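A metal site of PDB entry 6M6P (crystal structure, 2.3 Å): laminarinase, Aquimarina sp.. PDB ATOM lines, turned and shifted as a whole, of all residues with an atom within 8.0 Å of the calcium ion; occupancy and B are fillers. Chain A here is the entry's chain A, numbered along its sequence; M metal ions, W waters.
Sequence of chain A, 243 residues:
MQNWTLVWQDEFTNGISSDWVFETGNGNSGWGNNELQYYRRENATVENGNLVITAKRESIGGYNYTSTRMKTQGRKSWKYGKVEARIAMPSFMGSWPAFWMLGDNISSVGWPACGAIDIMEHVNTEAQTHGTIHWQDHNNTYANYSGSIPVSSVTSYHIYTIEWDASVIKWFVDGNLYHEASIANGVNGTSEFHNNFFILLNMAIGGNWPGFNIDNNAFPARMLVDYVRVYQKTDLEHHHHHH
OD2 of Asp 226 is in salt-bridge range of NH1 of Arg 86.
The guanidinium group (NH2) of Arg 229 lies within salt-bridge range of the side-chain carboxylate (OE1) of Glu 11 (2.8 Å).
Of the 18 residues printed, 3 come within 4 Å of the calcium ion.
The nearest printed residue that does not touch the calcium ion is Tyr 227 (4.4 Å).
The calcium ion is bound by O of Asp 226 (2.2 Å), O of Gly 49 (2.3 Å), O of Glu 11 (2.4 Å), OD1 of Asp 226 (2.6 Å) and water W1 (2.7 Å).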
ATOM      1  N   ASP A  10     -12.221 -19.034  -1.578  1.00  0.00           N
ATOM      2  CA  ASP A  10     -13.202 -19.175  -2.676  1.00  0.00           C
ATOM      3  C   ASP A  10     -12.474 -19.731  -3.907  1.00  0.00           C
ATOM      4  O   ASP A  10     -11.553 -19.068  -4.382  1.00  0.00           O
ATOM      5  CB  ASP A  10     -13.889 -17.849  -2.944  1.00  0.00           C
ATOM      6  CG  ASP A  10     -15.176 -18.023  -3.719  1.00  0.00           C
ATOM      7  OD1 ASP A  10     -15.354 -19.122  -4.313  1.00  0.00           O
ATOM      8  OD2 ASP A  10     -15.996 -17.069  -3.696  1.00  0.00           O
ATOM      9  N   GLU A  11     -12.847 -20.928  -4.367  1.00  0.00           N
ATOM     10  CA  GLU A  11     -12.290 -21.547  -5.593  1.00  0.00           C
ATOM     11  C   GLU A  11     -13.182 -21.176  -6.770  1.00  0.00           C
ATOM     12  O   GLU A  11     -12.794 -21.501  -7.926  1.00  0.00           O
ATOM     13  CB  GLU A  11     -12.149 -23.069  -5.473  1.00  0.00           C
ATOM     14  CG  GLU A  11     -11.320 -23.536  -4.284  1.00  0.00           C
ATOM     15  CD  GLU A  11      -9.885 -23.056  -4.254  1.00  0.00           C
ATOM     16  OE1 GLU A  11      -9.194 -23.189  -5.265  1.00  0.00           O
ATOM     17  OE2 GLU A  11      -9.464 -22.538  -3.219  1.00  0.00           O
ATOM     18  N   PHE A  12     -14.329 -20.531  -6.514  1.00  0.00           N
ATOM     19  CA  PHE A  12     -15.310 -20.106  -7.548  1.00  0.00           C
ATOM     20  C   PHE A  12     -15.770 -21.324  -8.376  1.00  0.00           C
ATOM     21  O   PHE A  12     -16.171 -21.132  -9.540  1.00  0.00           O
ATOM     22  CB  PHE A  12     -14.679 -19.068  -8.482  1.00  0.00           C
ATOM     23  CG  PHE A  12     -14.143 -17.870  -7.755  1.00  0.00           C
ATOM     24  CD1 PHE A  12     -15.015 -17.029  -7.082  1.00  0.00           C
ATOM     25  CD2 PHE A  12     -12.789 -17.588  -7.718  1.00  0.00           C
ATOM     26  CE1 PHE A  12     -14.541 -15.919  -6.397  1.00  0.00           C
ATOM     27  CE2 PHE A  12     -12.321 -16.491  -7.036  1.00  0.00           C
ATOM     28  CZ  PHE A  12     -13.195 -15.670  -6.371  1.00  0.00           C
ATOM     29  N   THR A  13     -15.723 -22.526  -7.790  1.00  0.00           N
ATOM     30  CA  THR A  13     -15.948 -23.792  -8.533  1.00  0.00           C
ATOM     31  C   THR A  13     -17.433 -23.899  -8.884  1.00  0.00           C
ATOM     32  O   THR A  13     -17.723 -23.991 -10.094  1.00  0.00           O
ATOM     33  CB  THR A  13     -15.399 -24.999  -7.782  1.00  0.00           C
ATOM     34  OG1 THR A  13     -15.694 -24.794  -6.412  1.00  0.00           O
ATOM     35  CG2 THR A  13     -13.905 -25.136  -7.916  1.00  0.00           C
ATOM     36  N   ASN A  14     -18.334 -23.757  -7.915  1.00  0.00           N
ATOM     37  CA  ASN A  14     -19.790 -23.643  -8.247  1.00  0.00           C
ATOM     38  C   ASN A  14     -20.030 -22.218  -8.787  1.00  0.00           C
ATOM     39  O   ASN A  14     -19.914 -22.002 -10.017  1.00  0.00           O
ATOM     40  CB  ASN A  14     -20.677 -24.131  -7.092  1.00  0.00           C
ATOM     41  CG  ASN A  14     -20.670 -23.248  -5.865  1.00  0.00           C
ATOM     42  OD1 ASN A  14     -20.047 -22.185  -5.864  1.00  0.00           O
ATOM     43  ND2 ASN A  14     -21.374 -23.653  -4.823  1.00  0.00           N
ATOM     44  N   VAL A  46     -19.114 -16.215 -13.357  1.00  0.00           N
ATOM     45  CA  VAL A  46     -18.173 -17.350 -13.190  1.00  0.00           C
ATOM     46  C   VAL A  46     -18.152 -18.107 -14.508  1.00  0.00           C
ATOM     47  O   VAL A  46     -19.226 -18.347 -15.074  1.00  0.00           O
ATOM     48  CB  VAL A  46     -18.562 -18.229 -11.992  1.00  0.00           C
ATOM     49  CG1 VAL A  46     -17.754 -19.533 -11.948  1.00  0.00           C
ATOM     50  CG2 VAL A  46     -18.409 -17.466 -10.683  1.00  0.00           C
ATOM     51  N   GLU A  47     -16.956 -18.463 -14.972  1.00  0.00           N
ATOM     52  CA  GLU A  47     -16.763 -19.351 -16.129  1.00  0.00           C
ATOM     53  C   GLU A  47     -15.663 -20.359 -15.788  1.00  0.00           C
ATOM     54  O   GLU A  47     -14.555 -19.933 -15.414  1.00  0.00           O
ATOM     55  CB  GLU A  47     -16.352 -18.550 -17.369  1.00  0.00           C
ATOM     56  CG  GLU A  47     -17.239 -17.346 -17.659  1.00  0.00           C
ATOM     57  CD  GLU A  47     -16.796 -16.588 -18.906  1.00  0.00           C
ATOM     58  OE1 GLU A  47     -15.843 -17.067 -19.572  1.00  0.00           O
ATOM     59  OE2 GLU A  47     -17.403 -15.531 -19.226  1.00  0.00           O
ATOM     60  N   ASN A  48     -15.973 -21.650 -15.888  1.00  0.00           N
ATOM     61  CA  ASN A  48     -15.005 -22.755 -15.752  1.00  0.00           C
ATOM     62  C   ASN A  48     -14.140 -22.547 -14.495  1.00  0.00           C
ATOM     63  O   ASN A  48     -12.939 -22.648 -14.587  1.00  0.00           O
ATOM     64  CB  ASN A  48     -14.142 -22.908 -17.009  1.00  0.00           C
ATOM     65  CG  ASN A  48     -13.547 -24.303 -17.073  1.00  0.00           C
ATOM     66  OD1 ASN A  48     -14.120 -25.248 -16.515  1.00  0.00           O
ATOM     67  ND2 ASN A  48     -12.388 -24.464 -17.712  1.00  0.00           N
ATOM     68  N   GLY A  49     -14.764 -22.315 -13.349  1.00  0.00           N
ATOM     69  CA  GLY A  49     -14.047 -22.323 -12.059  1.00  0.00           C
ATOM     70  C   GLY A  49     -13.317 -21.012 -11.812  1.00  0.00           C
ATOM     71  O   GLY A  49     -12.555 -20.958 -10.852  1.00  0.00           O
ATOM     72  N   ASN A  50     -13.553 -19.979 -12.628  1.00  0.00           N
ATOM     73  CA  ASN A  50     -12.909 -18.648 -12.459  1.00  0.00           C
ATOM     74  C   ASN A  50     -13.973 -17.580 -12.216  1.00  0.00           C
ATOM     75  O   ASN A  50     -14.988 -17.564 -12.927  1.00  0.00           O
ATOM     76  CB  ASN A  50     -12.046 -18.285 -13.673  1.00  0.00           C
ATOM     77  CG  ASN A  50     -10.804 -19.137 -13.776  1.00  0.00           C
ATOM     78  OD1 ASN A  50      -9.690 -18.620 -13.661  1.00  0.00           O
ATOM     79  ND2 ASN A  50     -10.969 -20.424 -13.967  1.00  0.00           N
ATOM     80  N   LEU A  51     -13.719 -16.673 -11.275  1.00  0.00           N
ATOM     81  CA  LEU A  51     -14.438 -15.384 -11.184  1.00  0.00           C
ATOM     82  C   LEU A  51     -14.052 -14.550 -12.413  1.00  0.00           C
ATOM     83  O   LEU A  51     -12.877 -14.551 -12.806  1.00  0.00           O
ATOM     84  CB  LEU A  51     -14.061 -14.712  -9.873  1.00  0.00           C
ATOM     85  CG  LEU A  51     -14.414 -13.226  -9.746  1.00  0.00           C
ATOM     86  CD1 LEU A  51     -15.925 -12.999  -9.567  1.00  0.00           C
ATOM     87  CD2 LEU A  51     -13.662 -12.642  -8.561  1.00  0.00           C
ATOM     88  N   ARG A  86      -4.759 -16.123  -7.402  1.00  0.00           N
ATOM     89  CA  ARG A  86      -4.245 -16.386  -8.766  1.00  0.00           C
ATOM     90  C   ARG A  86      -5.102 -15.585  -9.743  1.00  0.00           C
ATOM     91  O   ARG A  86      -6.303 -15.847  -9.832  1.00  0.00           O
ATOM     92  CB  ARG A  86      -4.262 -17.878  -9.026  1.00  0.00           C
ATOM     93  CG  ARG A  86      -3.660 -18.269 -10.360  1.00  0.00           C
ATOM     94  CD  ARG A  86      -3.378 -19.747 -10.381  1.00  0.00           C
ATOM     95  NE  ARG A  86      -2.668 -20.059 -11.602  1.00  0.00           N
ATOM     96  CZ  ARG A  86      -3.210 -20.594 -12.696  1.00  0.00           C
ATOM     97  NH1 ARG A  86      -4.492 -20.931 -12.735  1.00  0.00           N
ATOM     98  NH2 ARG A  86      -2.442 -20.803 -13.754  1.00  0.00           N
ATOM     99  N   TYR A 157      -2.074 -15.714 -15.984  1.00  0.00           N
ATOM    100  CA  TYR A 157      -2.225 -15.993 -14.543  1.00  0.00           C
ATOM    101  C   TYR A 157      -0.873 -15.790 -13.856  1.00  0.00           C
ATOM    102  O   TYR A 157       0.160 -16.320 -14.332  1.00  0.00           O
ATOM    103  CB  TYR A 157      -2.755 -17.411 -14.263  1.00  0.00           C
ATOM    104  CG  TYR A 157      -4.206 -17.616 -14.634  1.00  0.00           C
ATOM    105  CD1 TYR A 157      -5.246 -16.997 -13.935  1.00  0.00           C
ATOM    106  CD2 TYR A 157      -4.550 -18.433 -15.689  1.00  0.00           C
ATOM    107  CE1 TYR A 157      -6.568 -17.209 -14.283  1.00  0.00           C
ATOM    108  CE2 TYR A 157      -5.862 -18.646 -16.051  1.00  0.00           C
ATOM    109  CZ  TYR A 157      -6.884 -18.042 -15.353  1.00  0.00           C
ATOM    110  OH  TYR A 157      -8.168 -18.300 -15.767  1.00  0.00           O
ATOM    111  N   VAL A 225     -10.076 -14.453 -11.917  1.00  0.00           N
ATOM    112  CA  VAL A 225      -9.543 -14.879 -10.591  1.00  0.00           C
ATOM    113  C   VAL A 225      -9.826 -16.377 -10.460  1.00  0.00           C
ATOM    114  O   VAL A 225     -10.984 -16.748 -10.327  1.00  0.00           O
ATOM    115  CB  VAL A 225     -10.144 -14.050  -9.441  1.00  0.00           C
ATOM    116  CG1 VAL A 225      -9.502 -14.398  -8.105  1.00  0.00           C
ATOM    117  CG2 VAL A 225      -9.997 -12.559  -9.724  1.00  0.00           C
ATOM    118  N   ASP A 226      -8.778 -17.198 -10.567  1.00  0.00           N
ATOM    119  CA  ASP A 226      -8.850 -18.660 -10.386  1.00  0.00           C
ATOM    120  C   ASP A 226      -9.283 -18.936  -8.943  1.00  0.00           C
ATOM    121  O   ASP A 226     -10.147 -19.823  -8.744  1.00  0.00           O
ATOM    122  CB  ASP A 226      -7.538 -19.326 -10.761  1.00  0.00           C
ATOM    123  CG  ASP A 226      -7.626 -20.842 -10.861  1.00  0.00           C
ATOM    124  OD1 ASP A 226      -8.756 -21.352 -10.786  1.00  0.00           O
ATOM    125  OD2 ASP A 226      -6.546 -21.504 -10.988  1.00  0.00           O
ATOM    126  N   TYR A 227      -8.699 -18.259  -7.959  1.00  0.00           N
ATOM    127  CA  TYR A 227      -9.029 -18.519  -6.532  1.00  0.00           C
ATOM    128  C   TYR A 227      -8.545 -17.381  -5.632  1.00  0.00           C
ATOM    129  O   TYR A 227      -7.705 -16.625  -6.029  1.00  0.00           O
ATOM    130  CB  TYR A 227      -8.414 -19.840  -6.090  1.00  0.00           C
ATOM    131  CG  TYR A 227      -6.913 -19.906  -6.151  1.00  0.00           C
ATOM    132  CD1 TYR A 227      -6.127 -19.264  -5.213  1.00  0.00           C
ATOM    133  CD2 TYR A 227      -6.272 -20.661  -7.122  1.00  0.00           C
ATOM    134  CE1 TYR A 227      -4.747 -19.330  -5.257  1.00  0.00           C
ATOM    135  CE2 TYR A 227      -4.890 -20.776  -7.164  1.00  0.00           C
ATOM    136  CZ  TYR A 227      -4.121 -20.102  -6.230  1.00  0.00           C
ATOM    137  OH  TYR A 227      -2.766 -20.205  -6.271  1.00  0.00           O
ATOM    138  N   VAL A 228      -9.126 -17.274  -4.452  1.00  0.00           N
ATOM    139  CA  VAL A 228      -8.582 -16.501  -3.300  1.00  0.00           C
ATOM    140  C   VAL A 228      -8.471 -17.437  -2.083  1.00  0.00           C
ATOM    141  O   VAL A 228      -9.390 -18.260  -1.883  1.00  0.00           O
ATOM    142  CB  VAL A 228      -9.457 -15.279  -2.993  1.00  0.00           C
ATOM    143  CG1 VAL A 228      -8.819 -14.378  -1.952  1.00  0.00           C
ATOM    144  CG2 VAL A 228      -9.741 -14.505  -4.271  1.00  0.00           C
ATOM    145  N   ARG A 229      -7.376 -17.307  -1.310  1.00  0.00           N
ATOM    146  CA  ARG A 229      -7.075 -18.246  -0.202  1.00  0.00           C
ATOM    147  C   ARG A 229      -6.424 -17.507   0.958  1.00  0.00           C
ATOM    148  O   ARG A 229      -5.597 -16.642   0.727  1.00  0.00           O
ATOM    149  CB  ARG A 229      -6.196 -19.382  -0.699  1.00  0.00           C
ATOM    150  CG  ARG A 229      -6.901 -20.312  -1.675  1.00  0.00           C
ATOM    151  CD  ARG A 229      -5.901 -21.246  -2.305  1.00  0.00           C
ATOM    152  NE  ARG A 229      -6.488 -22.047  -3.354  1.00  0.00           N
ATOM    153  CZ  ARG A 229      -5.797 -22.863  -4.140  1.00  0.00           C
ATOM    154  NH1 ARG A 229      -4.491 -22.985  -3.990  1.00  0.00           N
ATOM    155  NH2 ARG A 229      -6.403 -23.552  -5.076  1.00  0.00           N
HETATM  156 CA    CA M   1     -10.908 -21.767  -9.428  1.00  0.00          CA
HETATM  157  O   HOH W   1      -9.393 -23.564  -8.007  1.00  0.00           O
